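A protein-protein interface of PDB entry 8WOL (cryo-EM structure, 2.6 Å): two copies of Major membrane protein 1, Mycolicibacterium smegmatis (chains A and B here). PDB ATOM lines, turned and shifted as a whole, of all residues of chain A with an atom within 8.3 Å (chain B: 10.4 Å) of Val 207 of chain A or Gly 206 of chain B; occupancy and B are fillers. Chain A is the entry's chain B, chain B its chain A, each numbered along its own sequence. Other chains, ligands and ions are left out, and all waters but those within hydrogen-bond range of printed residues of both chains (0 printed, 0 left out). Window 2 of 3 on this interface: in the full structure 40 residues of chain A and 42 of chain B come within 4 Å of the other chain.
Of the 17 printed residues of chain B, 5 touch a printed residue of chain A.
Hydrophobic or aromatic side chains of chain B within 4 Å of the printed part of chain A: Pro 209 and Tyr 315.
Of the 18 printed residues of chain A, 3 touch a printed residue of chain B.
Among the printed residues, 5 pairs touch across the chains.
Among the printed residues, no Asp or Glu carboxylate lies within 4 Å of a Lys or Arg side-chain nitrogen of the other chain.
Printed residues of chain B within 4 Å of Arg 205 of chain A: Tyr 315 (3.6 Å).
No residue of chain B comes within 4 Å of Gly 206 of chain A.
Of the printed residues of chain B, Val 207 of chain A touches Gly 206.
No residue of chain B comes within 4 Å of Pro 208 of chain A.
No residue of chain B comes within 4 Å of Pro 209 of chain A.
Printed residues of chain B within 4 Å of Arg 223 of chain A: Gly 199 (3.5 Å), Thr 203 (3.8 Å) and Pro 209 (3.9 Å).
Of the printed residues of chain A, Gly 199 of chain B touches Arg 223 (3.5 Å).
Printed residues of chain A within 4 Å of Gly 206 of chain B: Val 207 (3.99 Å).
Of the printed residues of chain A, Pro 209 of chain B touches Arg 223 (3.9 Å).
The nearest printed residue of chain B that does not touch Val 207 of chain A is Pro 208 of chain B (4.01 Å).
The nearest printed residue of chain A that does not touch Gly 206 of chain B is Arg 205 of chain A (4.4 Å).
The nearest printed residue of chain A that does not touch Pro 209 of chain B is Pro 210 of chain A (6.9 Å).
The side-chain hydroxyl (OG1) of Thr 203 of chain B sits at hydrogen-bond distance from the backbone carbonyl oxygen (O) of Gly 199 of chain B (3.0 Å).
The side-chain carboxylate (OE2) of Glu 201 of chain A is in salt-bridge range of the guanidinium group (NH1) of Arg 205 of chain A.
The backbone carbonyl oxygen (O) of Cys 202 of chain A lies within hydrogen-bond range of the backbone NH (N) of Val 207 of chain A (3.2 Å).
Val 207 of chain A touches Gly 206 of chain B, but with the chains exchanged Gly 206 of chain A does not touch Val 207 of chain B (5.8 Å).
Positions printed for both chains: 171, 198, 199, 200, 201, 202, 203, 204, 205, 206, 207, 208, 209, 210 and 222.
Of the 5 pairs that touch across the chains among the printed residues, none has its exchanged pair printed and touching as well.
Arg 205 of chain A touches Tyr 315 of chain B.
Gly 206 of chain B touches Val 207 of chain A.
CA of Gly 199 of chain B touches NH2 of Arg 223 of chain A, 3.5 Å away.
Thr 203 of chain B touches Arg 223 of chain A (OG1 to NH2, 3.8 Å).
NH1 of Arg 223 of chain A touches CD of Pro 209 of chain B (3.9 Å).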
ATOM      1  N   PRO A 171      -7.340  14.108  -7.773  1.00  0.00           N
ATOM      2  CA  PRO A 171      -6.346  15.195  -7.844  1.00  0.00           C
ATOM      3  C   PRO A 171      -5.275  15.122  -6.767  1.00  0.00           C
ATOM      4  O   PRO A 171      -4.121  15.493  -7.017  1.00  0.00           O
ATOM      5  CB  PRO A 171      -7.214  16.449  -7.690  1.00  0.00           C
ATOM      6  CG  PRO A 171      -8.517  16.070  -8.288  1.00  0.00           C
ATOM      7  CD  PRO A 171      -8.704  14.592  -8.052  1.00  0.00           C
ATOM      8  N   PHE A 198     -10.126   9.477 -14.201  1.00  0.00           N
ATOM      9  CA  PHE A 198      -9.649  10.745 -13.659  1.00  0.00           C
ATOM     10  C   PHE A 198     -10.594  11.884 -14.016  1.00  0.00           C
ATOM     11  O   PHE A 198     -10.830  12.782 -13.201  1.00  0.00           O
ATOM     12  CB  PHE A 198      -8.236  11.039 -14.159  1.00  0.00           C
ATOM     13  CG  PHE A 198      -7.677  12.339 -13.654  1.00  0.00           C
ATOM     14  CD1 PHE A 198      -7.387  12.505 -12.309  1.00  0.00           C
ATOM     15  CD2 PHE A 198      -7.440  13.393 -14.520  1.00  0.00           C
ATOM     16  CE1 PHE A 198      -6.875  13.697 -11.837  1.00  0.00           C
ATOM     17  CE2 PHE A 198      -6.926  14.590 -14.054  1.00  0.00           C
ATOM     18  CZ  PHE A 198      -6.643  14.742 -12.712  1.00  0.00           C
ATOM     19  N   GLY A 199     -11.133  11.873 -15.237  1.00  0.00           N
ATOM     20  CA  GLY A 199     -12.122  12.872 -15.605  1.00  0.00           C
ATOM     21  C   GLY A 199     -13.372  12.793 -14.749  1.00  0.00           C
ATOM     22  O   GLY A 199     -13.922  13.818 -14.342  1.00  0.00           O
ATOM     23  N   ARG A 200     -13.834  11.573 -14.462  1.00  0.00           N
ATOM     24  CA  ARG A 200     -14.983  11.407 -13.576  1.00  0.00           C
ATOM     25  C   ARG A 200     -14.688  11.954 -12.185  1.00  0.00           C
ATOM     26  O   ARG A 200     -15.519  12.657 -11.592  1.00  0.00           O
ATOM     27  CB  ARG A 200     -15.372   9.931 -13.492  1.00  0.00           C
ATOM     28  CG  ARG A 200     -16.046   9.376 -14.733  1.00  0.00           C
ATOM     29  CD  ARG A 200     -16.859   8.136 -14.401  1.00  0.00           C
ATOM     30  NE  ARG A 200     -16.044   7.084 -13.801  1.00  0.00           N
ATOM     31  CZ  ARG A 200     -15.224   6.290 -14.475  1.00  0.00           C
ATOM     32  NH1 ARG A 200     -15.082   6.391 -15.786  1.00  0.00           N
ATOM     33  NH2 ARG A 200     -14.529   5.367 -13.815  1.00  0.00           N
ATOM     34  N   GLU A 201     -13.506  11.640 -11.647  1.00  0.00           N
ATOM     35  CA  GLU A 201     -13.141  12.129 -10.320  1.00  0.00           C
ATOM     36  C   GLU A 201     -13.018  13.647 -10.291  1.00  0.00           C
ATOM     37  O   GLU A 201     -13.387  14.279  -9.294  1.00  0.00           O
ATOM     38  CB  GLU A 201     -11.836  11.479  -9.857  1.00  0.00           C
ATOM     39  CG  GLU A 201     -11.966  10.025  -9.413  1.00  0.00           C
ATOM     40  CD  GLU A 201     -13.074   9.805  -8.397  1.00  0.00           C
ATOM     41  OE1 GLU A 201     -14.235   9.598  -8.806  1.00  0.00           O
ATOM     42  OE2 GLU A 201     -12.782   9.840  -7.183  1.00  0.00           O
ATOM     43  N   CYS A 202     -12.500  14.249 -11.364  1.00  0.00           N
ATOM     44  CA  CYS A 202     -12.436  15.704 -11.442  1.00  0.00           C
ATOM     45  C   CYS A 202     -13.829  16.311 -11.537  1.00  0.00           C
ATOM     46  O   CYS A 202     -14.094  17.369 -10.956  1.00  0.00           O
ATOM     47  CB  CYS A 202     -11.585  16.130 -12.639  1.00  0.00           C
ATOM     48  SG  CYS A 202      -9.806  16.130 -12.338  1.00  0.00           S
ATOM     49  N   THR A 203     -14.727  15.658 -12.277  1.00  0.00           N
ATOM     50  CA  THR A 203     -16.092  16.154 -12.408  1.00  0.00           C
ATOM     51  C   THR A 203     -16.824  16.112 -11.073  1.00  0.00           C
ATOM     52  O   THR A 203     -17.593  17.025 -10.748  1.00  0.00           O
ATOM     53  CB  THR A 203     -16.840  15.337 -13.463  1.00  0.00           C
ATOM     54  OG1 THR A 203     -16.279  15.596 -14.756  1.00  0.00           O
ATOM     55  CG2 THR A 203     -18.319  15.697 -13.481  1.00  0.00           C
ATOM     56  N   TYR A 204     -16.589  15.063 -10.278  1.00  0.00           N
ATOM     57  CA  TYR A 204     -17.277  14.947  -8.996  1.00  0.00           C
ATOM     58  C   TYR A 204     -16.930  16.093  -8.053  1.00  0.00           C
ATOM     59  O   TYR A 204     -17.759  16.484  -7.224  1.00  0.00           O
ATOM     60  CB  TYR A 204     -16.946  13.610  -8.337  1.00  0.00           C
ATOM     61  CG  TYR A 204     -17.701  13.375  -7.050  1.00  0.00           C
ATOM     62  CD1 TYR A 204     -19.081  13.231  -7.049  1.00  0.00           C
ATOM     63  CD2 TYR A 204     -17.034  13.307  -5.834  1.00  0.00           C
ATOM     64  CE1 TYR A 204     -19.776  13.017  -5.876  1.00  0.00           C
ATOM     65  CE2 TYR A 204     -17.721  13.094  -4.656  1.00  0.00           C
ATOM     66  CZ  TYR A 204     -19.091  12.950  -4.681  1.00  0.00           C
ATOM     67  OH  TYR A 204     -19.776  12.738  -3.508  1.00  0.00           O
ATOM     68  N   ARG A 205     -15.722  16.638  -8.157  1.00  0.00           N
ATOM     69  CA  ARG A 205     -15.293  17.744  -7.310  1.00  0.00           C
ATOM     70  C   ARG A 205     -15.504  19.108  -7.954  1.00  0.00           C
ATOM     71  O   ARG A 205     -15.153  20.124  -7.344  1.00  0.00           O
ATOM     72  CB  ARG A 205     -13.819  17.579  -6.928  1.00  0.00           C
ATOM     73  CG  ARG A 205     -13.560  16.488  -5.903  1.00  0.00           C
ATOM     74  CD  ARG A 205     -12.255  15.759  -6.175  1.00  0.00           C
ATOM     75  NE  ARG A 205     -12.015  14.702  -5.201  1.00  0.00           N
ATOM     76  CZ  ARG A 205     -12.456  13.457  -5.318  1.00  0.00           C
ATOM     77  NH1 ARG A 205     -13.161  13.069  -6.368  1.00  0.00           N
ATOM     78  NH2 ARG A 205     -12.185  12.580  -4.356  1.00  0.00           N
ATOM     79  N   GLY A 206     -16.065  19.159  -9.157  1.00  0.00           N
ATOM     80  CA  GLY A 206     -16.316  20.428  -9.821  1.00  0.00           C
ATOM     81  C   GLY A 206     -15.071  21.211 -10.177  1.00  0.00           C
ATOM     82  O   GLY A 206     -15.048  22.437 -10.008  1.00  0.00           O
ATOM     83  N   VAL A 207     -14.034  20.537 -10.664  1.00  0.00           N
ATOM     84  CA  VAL A 207     -12.793  21.201 -11.056  1.00  0.00           C
ATOM     85  C   VAL A 207     -12.423  20.781 -12.476  1.00  0.00           C
ATOM     86  O   VAL A 207     -11.592  19.881 -12.664  1.00  0.00           O
ATOM     87  CB  VAL A 207     -11.659  20.901 -10.061  1.00  0.00           C
ATOM     88  CG1 VAL A 207     -11.772  21.813  -8.851  1.00  0.00           C
ATOM     89  CG2 VAL A 207     -11.702  19.445  -9.616  1.00  0.00           C
ATOM     90  N   PRO A 208     -13.003  21.404 -13.499  1.00  0.00           N
ATOM     91  CA  PRO A 208     -12.730  20.987 -14.878  1.00  0.00           C
ATOM     92  C   PRO A 208     -11.346  21.424 -15.320  1.00  0.00           C
ATOM     93  O   PRO A 208     -11.009  22.618 -15.264  1.00  0.00           O
ATOM     94  CB  PRO A 208     -13.827  21.697 -15.681  1.00  0.00           C
ATOM     95  CG  PRO A 208     -14.142  22.918 -14.885  1.00  0.00           C
ATOM     96  CD  PRO A 208     -13.888  22.582 -13.434  1.00  0.00           C
ATOM     97  N   PRO A 209     -10.512  20.489 -15.764  1.00  0.00           N
ATOM     98  CA  PRO A 209      -9.156  20.839 -16.193  1.00  0.00           C
ATOM     99  C   PRO A 209      -9.140  21.309 -17.636  1.00  0.00           C
ATOM    100  O   PRO A 209      -9.936  20.838 -18.463  1.00  0.00           O
ATOM    101  CB  PRO A 209      -8.386  19.522 -16.029  1.00  0.00           C
ATOM    102  CG  PRO A 209      -9.421  18.468 -16.213  1.00  0.00           C
ATOM    103  CD  PRO A 209     -10.730  19.031 -15.731  1.00  0.00           C
ATOM    104  N   PRO A 210      -8.246  22.239 -17.981  1.00  0.00           N
ATOM    105  CA  PRO A 210      -8.147  22.689 -19.378  1.00  0.00           C
ATOM    106  C   PRO A 210      -7.487  21.655 -20.278  1.00  0.00           C
ATOM    107  O   PRO A 210      -7.026  20.613 -19.805  1.00  0.00           O
ATOM    108  CB  PRO A 210      -7.303  23.967 -19.279  1.00  0.00           C
ATOM    109  CG  PRO A 210      -6.534  23.825 -18.018  1.00  0.00           C
ATOM    110  CD  PRO A 210      -7.365  23.003 -17.080  1.00  0.00           C
ATOM    111  N   ILE A 220      -5.860  16.376 -21.877  1.00  0.00           N
ATOM    112  CA  ILE A 220      -6.177  16.940 -20.572  1.00  0.00           C
ATOM    113  C   ILE A 220      -4.888  17.213 -19.809  1.00  0.00           C
ATOM    114  O   ILE A 220      -3.986  16.365 -19.751  1.00  0.00           O
ATOM    115  CB  ILE A 220      -7.099  15.987 -19.791  1.00  0.00           C
ATOM    116  CG1 ILE A 220      -8.442  15.836 -20.508  1.00  0.00           C
ATOM    117  CG2 ILE A 220      -7.290  16.468 -18.362  1.00  0.00           C
ATOM    118  CD1 ILE A 220      -9.355  17.027 -20.335  1.00  0.00           C
ATOM    119  N   THR A 221      -4.789  18.402 -19.221  1.00  0.00           N
ATOM    120  CA  THR A 221      -3.622  18.796 -18.447  1.00  0.00           C
ATOM    121  C   THR A 221      -4.001  18.969 -16.983  1.00  0.00           C
ATOM    122  O   THR A 221      -5.086  19.460 -16.658  1.00  0.00           O
ATOM    123  CB  THR A 221      -3.007  20.102 -18.972  1.00  0.00           C
ATOM    124  OG1 THR A 221      -3.884  21.197 -18.676  1.00  0.00           O
ATOM    125  CG2 THR A 221      -2.784  20.025 -20.476  1.00  0.00           C
ATOM    126  N   TRP A 222      -3.090  18.562 -16.101  1.00  0.00           N
ATOM    127  CA  TRP A 222      -3.235  18.764 -14.666  1.00  0.00           C
ATOM    128  C   TRP A 222      -2.022  19.536 -14.173  1.00  0.00           C
ATOM    129  O   TRP A 222      -0.890  19.053 -14.287  1.00  0.00           O
ATOM    130  CB  TRP A 222      -3.368  17.433 -13.918  1.00  0.00           C
ATOM    131  CG  TRP A 222      -3.575  17.617 -12.448  1.00  0.00           C
ATOM    132  CD1 TRP A 222      -2.726  17.244 -11.449  1.00  0.00           C
ATOM    133  CD2 TRP A 222      -4.701  18.231 -11.810  1.00  0.00           C
ATOM    134  NE1 TRP A 222      -3.254  17.585 -10.227  1.00  0.00           N
ATOM    135  CE2 TRP A 222      -4.466  18.192 -10.422  1.00  0.00           C
ATOM    136  CE3 TRP A 222      -5.885  18.808 -12.277  1.00  0.00           C
ATOM    137  CZ2 TRP A 222      -5.369  18.709  -9.499  1.00  0.00           C
ATOM    138  CZ3 TRP A 222      -6.781  19.318 -11.358  1.00  0.00           C
ATOM    139  CH2 TRP A 222      -6.519  19.266  -9.984  1.00  0.00           C
ATOM    140  N   ARG A 223      -2.263  20.731 -13.631  1.00  0.00           N
ATOM    141  CA  ARG A 223      -1.205  21.647 -13.203  1.00  0.00           C
ATOM    142  C   ARG A 223      -0.252  21.984 -14.347  1.00  0.00           C
ATOM    143  O   ARG A 223       0.938  22.219 -14.129  1.00  0.00           O
ATOM    144  CB  ARG A 223      -0.428  21.088 -12.007  1.00  0.00           C
ATOM    145  CG  ARG A 223      -1.299  20.496 -10.912  1.00  0.00           C
ATOM    146  CD  ARG A 223      -2.206  21.551 -10.306  1.00  0.00           C
ATOM    147  NE  ARG A 223      -2.776  21.120  -9.035  1.00  0.00           N
ATOM    148  CZ  ARG A 223      -3.857  21.650  -8.481  1.00  0.00           C
ATOM    149  NH1 ARG A 223      -4.522  22.635  -9.064  1.00  0.00           N
ATOM    150  NH2 ARG A 223      -4.285  21.180  -7.314  1.00  0.00           N
ATOM    151  N   PRO B 171      -6.748  29.643   0.724  1.00  0.00           N
ATOM    152  CA  PRO B 171      -6.787  30.911  -0.024  1.00  0.00           C
ATOM    153  C   PRO B 171      -6.889  32.143   0.861  1.00  0.00           C
ATOM    154  O   PRO B 171      -6.333  33.193   0.511  1.00  0.00           O
ATOM    155  CB  PRO B 171      -8.034  30.748  -0.901  1.00  0.00           C
ATOM    156  CG  PRO B 171      -8.115  29.288  -1.152  1.00  0.00           C
ATOM    157  CD  PRO B 171      -7.554  28.596   0.069  1.00  0.00           C
ATOM    158  N   PHE B 198      -1.445  23.312  -0.643  1.00  0.00           N
ATOM    159  CA  PHE B 198      -2.259  24.413  -1.145  1.00  0.00           C
ATOM    160  C   PHE B 198      -3.159  23.954  -2.284  1.00  0.00           C
ATOM    161  O   PHE B 198      -4.315  24.383  -2.379  1.00  0.00           O
ATOM    162  CB  PHE B 198      -1.369  25.571  -1.594  1.00  0.00           C
ATOM    163  CG  PHE B 198      -2.132  26.731  -2.165  1.00  0.00           C
ATOM    164  CD1 PHE B 198      -2.999  27.462  -1.370  1.00  0.00           C
ATOM    165  CD2 PHE B 198      -1.982  27.094  -3.494  1.00  0.00           C
ATOM    166  CE1 PHE B 198      -3.707  28.530  -1.890  1.00  0.00           C
ATOM    167  CE2 PHE B 198      -2.686  28.162  -4.019  1.00  0.00           C
ATOM    168  CZ  PHE B 198      -3.549  28.880  -3.216  1.00  0.00           C
ATOM    169  N   GLY B 199      -2.646  23.090  -3.161  1.00  0.00           N
ATOM    170  CA  GLY B 199      -3.484  22.540  -4.214  1.00  0.00           C
ATOM    171  C   GLY B 199      -4.633  21.714  -3.670  1.00  0.00           C
ATOM    172  O   GLY B 199      -5.756  21.791  -4.170  1.00  0.00           O
ATOM    173  N   ARG B 200      -4.369  20.913  -2.633  1.00  0.00           N
ATOM    174  CA  ARG B 200      -5.437  20.145  -2.001  1.00  0.00           C
ATOM    175  C   ARG B 200      -6.498  21.064  -1.407  1.00  0.00           C
ATOM    176  O   ARG B 200      -7.702  20.828  -1.572  1.00  0.00           O
ATOM    177  CB  ARG B 200      -4.859  19.236  -0.917  1.00  0.00           C
ATOM    178  CG  ARG B 200      -4.109  18.020  -1.435  1.00  0.00           C
ATOM    179  CD  ARG B 200      -4.025  16.940  -0.371  1.00  0.00           C
ATOM    180  NE  ARG B 200      -3.397  17.424   0.853  1.00  0.00           N
ATOM    181  CZ  ARG B 200      -2.089  17.550   1.030  1.00  0.00           C
ATOM    182  NH1 ARG B 200      -1.228  17.231   0.078  1.00  0.00           N
ATOM    183  NH2 ARG B 200      -1.633  18.007   2.192  1.00  0.00           N
ATOM    184  N   GLU B 201      -6.066  22.120  -0.711  1.00  0.00           N
ATOM    185  CA  GLU B 201      -7.021  23.046  -0.109  1.00  0.00           C
ATOM    186  C   GLU B 201      -7.817  23.804  -1.165  1.00  0.00           C
ATOM    187  O   GLU B 201      -9.003  24.084  -0.959  1.00  0.00           O
ATOM    188  CB  GLU B 201      -6.296  24.021   0.821  1.00  0.00           C
ATOM    189  CG  GLU B 201      -5.736  23.379   2.086  1.00  0.00           C
ATOM    190  CD  GLU B 201      -6.812  22.772   2.973  1.00  0.00           C
ATOM    191  OE1 GLU B 201      -7.982  23.203   2.883  1.00  0.00           O
ATOM    192  OE2 GLU B 201      -6.488  21.858   3.760  1.00  0.00           O
ATOM    193  N   CYS B 202      -7.188  24.146  -2.291  1.00  0.00           N
ATOM    194  CA  CYS B 202      -7.919  24.778  -3.385  1.00  0.00           C
ATOM    195  C   CYS B 202      -8.920  23.813  -4.007  1.00  0.00           C
ATOM    196  O   CYS B 202     -10.028  24.212  -4.383  1.00  0.00           O
ATOM    197  CB  CYS B 202      -6.944  25.292  -4.443  1.00  0.00           C
ATOM    198  SG  CYS B 202      -6.276  26.931  -4.105  1.00  0.00           S
ATOM    199  N   THR B 203      -8.538  22.540  -4.134  1.00  0.00           N
ATOM    200  CA  THR B 203      -9.441  21.542  -4.697  1.00  0.00           C
ATOM    201  C   THR B 203     -10.655  21.332  -3.802  1.00  0.00           C
ATOM    202  O   THR B 203     -11.778  21.166  -4.295  1.00  0.00           O
ATOM    203  CB  THR B 203      -8.688  20.227  -4.911  1.00  0.00           C
ATOM    204  OG1 THR B 203      -7.750  20.380  -5.982  1.00  0.00           O
ATOM    205  CG2 THR B 203      -9.651  19.098  -5.249  1.00  0.00           C
ATOM    206  N   TYR B 204     -10.451  21.341  -2.481  1.00  0.00           N
ATOM    207  CA  TYR B 204     -11.567  21.128  -1.564  1.00  0.00           C
ATOM    208  C   TYR B 204     -12.641  22.200  -1.711  1.00  0.00           C
ATOM    209  O   TYR B 204     -13.828  21.919  -1.506  1.00  0.00           O
ATOM    210  CB  TYR B 204     -11.066  21.086  -0.123  1.00  0.00           C
ATOM    211  CG  TYR B 204     -12.153  20.783   0.881  1.00  0.00           C
ATOM    212  CD1 TYR B 204     -12.832  19.573   0.852  1.00  0.00           C
ATOM    213  CD2 TYR B 204     -12.504  21.710   1.853  1.00  0.00           C
ATOM    214  CE1 TYR B 204     -13.828  19.292   1.766  1.00  0.00           C
ATOM    215  CE2 TYR B 204     -13.498  21.436   2.772  1.00  0.00           C
ATOM    216  CZ  TYR B 204     -14.157  20.226   2.724  1.00  0.00           C
ATOM    217  OH  TYR B 204     -15.147  19.953   3.640  1.00  0.00           O
ATOM    218  N   ARG B 205     -12.253  23.425  -2.055  1.00  0.00           N
ATOM    219  CA  ARG B 205     -13.199  24.517  -2.235  1.00  0.00           C
ATOM    220  C   ARG B 205     -13.637  24.696  -3.684  1.00  0.00           C
ATOM    221  O   ARG B 205     -14.416  25.611  -3.969  1.00  0.00           O
ATOM    222  CB  ARG B 205     -12.601  25.826  -1.712  1.00  0.00           C
ATOM    223  CG  ARG B 205     -12.484  25.896  -0.197  1.00  0.00           C
ATOM    224  CD  ARG B 205     -11.238  26.648   0.237  1.00  0.00           C
ATOM    225  NE  ARG B 205     -11.145  26.745   1.689  1.00  0.00           N
ATOM    226  CZ  ARG B 205     -10.573  25.836   2.467  1.00  0.00           C
ATOM    227  NH1 ARG B 205     -10.021  24.744   1.965  1.00  0.00           N
ATOM    228  NH2 ARG B 205     -10.557  26.028   3.783  1.00  0.00           N
ATOM    229  N   GLY B 206     -13.161  23.856  -4.596  1.00  0.00           N
ATOM    230  CA  GLY B 206     -13.558  23.953  -5.990  1.00  0.00           C
ATOM    231  C   GLY B 206     -13.121  25.223  -6.686  1.00  0.00           C
ATOM    232  O   GLY B 206     -13.904  25.809  -7.444  1.00  0.00           O
ATOM    233  N   VAL B 207     -11.892  25.668  -6.448  1.00  0.00           N
ATOM    234  CA  VAL B 207     -11.370  26.876  -7.083  1.00  0.00           C
ATOM    235  C   VAL B 207     -10.027  26.562  -7.736  1.00  0.00           C
ATOM    236  O   VAL B 207      -8.969  26.866  -7.165  1.00  0.00           O
ATOM    237  CB  VAL B 207     -11.255  28.031  -6.075  1.00  0.00           C
ATOM    238  CG1 VAL B 207     -12.604  28.710  -5.903  1.00  0.00           C
ATOM    239  CG2 VAL B 207     -10.754  27.525  -4.728  1.00  0.00           C
ATOM    240  N   PRO B 208     -10.019  25.967  -8.926  1.00  0.00           N
ATOM    241  CA  PRO B 208      -8.752  25.591  -9.565  1.00  0.00           C
ATOM    242  C   PRO B 208      -8.008  26.812 -10.074  1.00  0.00           C
ATOM    243  O   PRO B 208      -8.556  27.608 -10.853  1.00  0.00           O
ATOM    244  CB  PRO B 208      -9.197  24.684 -10.719  1.00  0.00           C
ATOM    245  CG  PRO B 208     -10.572  25.152 -11.054  1.00  0.00           C
ATOM    246  CD  PRO B 208     -11.184  25.671  -9.777  1.00  0.00           C
ATOM    247  N   PRO B 209      -6.759  26.998  -9.658  1.00  0.00           N
ATOM    248  CA  PRO B 209      -5.989  28.160 -10.105  1.00  0.00           C
ATOM    249  C   PRO B 209      -5.344  27.906 -11.455  1.00  0.00           C
ATOM    250  O   PRO B 209      -4.993  26.762 -11.782  1.00  0.00           O
ATOM    251  CB  PRO B 209      -4.932  28.322  -9.005  1.00  0.00           C
ATOM    252  CG  PRO B 209      -4.732  26.942  -8.488  1.00  0.00           C
ATOM    253  CD  PRO B 209      -6.055  26.231  -8.614  1.00  0.00           C
ATOM    254  N   PRO B 210      -5.170  28.949 -12.271  1.00  0.00           N
ATOM    255  CA  PRO B 210      -4.475  28.777 -13.554  1.00  0.00           C
ATOM    256  C   PRO B 210      -2.976  28.585 -13.381  1.00  0.00           C
ATOM    257  O   PRO B 210      -2.461  28.642 -12.260  1.00  0.00           O
ATOM    258  CB  PRO B 210      -4.793  30.075 -14.307  1.00  0.00           C
ATOM    259  CG  PRO B 210      -5.126  31.064 -13.251  1.00  0.00           C
ATOM    260  CD  PRO B 210      -5.736  30.301 -12.116  1.00  0.00           C
ATOM    261  N   TRP B 222      -1.650  32.374  -7.899  1.00  0.00           N
ATOM    262  CA  TRP B 222      -2.763  32.803  -7.063  1.00  0.00           C
ATOM    263  C   TRP B 222      -2.884  34.314  -7.173  1.00  0.00           C
ATOM    264  O   TRP B 222      -1.938  35.041  -6.849  1.00  0.00           O
ATOM    265  CB  TRP B 222      -2.565  32.381  -5.605  1.00  0.00           C
ATOM    266  CG  TRP B 222      -3.712  32.770  -4.725  1.00  0.00           C
ATOM    267  CD1 TRP B 222      -3.686  33.658  -3.690  1.00  0.00           C
ATOM    268  CD2 TRP B 222      -5.060  32.293  -4.811  1.00  0.00           C
ATOM    269  NE1 TRP B 222      -4.933  33.761  -3.124  1.00  0.00           N
ATOM    270  CE2 TRP B 222      -5.793  32.933  -3.794  1.00  0.00           C
ATOM    271  CE3 TRP B 222      -5.716  31.385  -5.647  1.00  0.00           C
ATOM    272  CZ2 TRP B 222      -7.151  32.697  -3.592  1.00  0.00           C
ATOM    273  CZ3 TRP B 222      -7.062  31.151  -5.444  1.00  0.00           C
ATOM    274  CH2 TRP B 222      -7.765  31.803  -4.425  1.00  0.00           C
ATOM    275  N   HIS B 313      -8.455  15.827   3.104  1.00  0.00           N
ATOM    276  CA  HIS B 313      -9.906  15.928   3.173  1.00  0.00           C
ATOM    277  C   HIS B 313     -10.559  14.630   2.710  1.00  0.00           C
ATOM    278  O   HIS B 313      -9.944  13.798   2.039  1.00  0.00           O
ATOM    279  CB  HIS B 313     -10.410  17.096   2.321  1.00  0.00           C
ATOM    280  CG  HIS B 313     -10.225  18.435   2.962  1.00  0.00           C
ATOM    281  ND1 HIS B 313     -11.014  18.880   4.001  1.00  0.00           N
ATOM    282  CD2 HIS B 313      -9.345  19.430   2.707  1.00  0.00           C
ATOM    283  CE1 HIS B 313     -10.624  20.089   4.361  1.00  0.00           C
ATOM    284  NE2 HIS B 313      -9.613  20.447   3.591  1.00  0.00           N
ATOM    285  N   TYR B 315     -14.101  12.740   0.922  1.00  0.00           N
ATOM    286  CA  TYR B 315     -15.176  12.930  -0.053  1.00  0.00           C
ATOM    287  C   TYR B 315     -16.096  11.714   0.013  1.00  0.00           C
ATOM    288  O   TYR B 315     -15.891  10.729  -0.702  1.00  0.00           O
ATOM    289  CB  TYR B 315     -14.617  13.135  -1.460  1.00  0.00           C
ATOM    290  CG  TYR B 315     -13.728  14.348  -1.604  1.00  0.00           C
ATOM    291  CD1 TYR B 315     -12.390  14.302  -1.238  1.00  0.00           C
ATOM    292  CD2 TYR B 315     -14.227  15.540  -2.110  1.00  0.00           C
ATOM    293  CE1 TYR B 315     -11.574  15.407  -1.371  1.00  0.00           C
ATOM    294  CE2 TYR B 315     -13.420  16.652  -2.247  1.00  0.00           C
ATOM    295  CZ  TYR B 315     -12.095  16.580  -1.875  1.00  0.00           C
ATOM    296  OH  TYR B 315     -11.289  17.685  -2.011  1.00  0.00           O
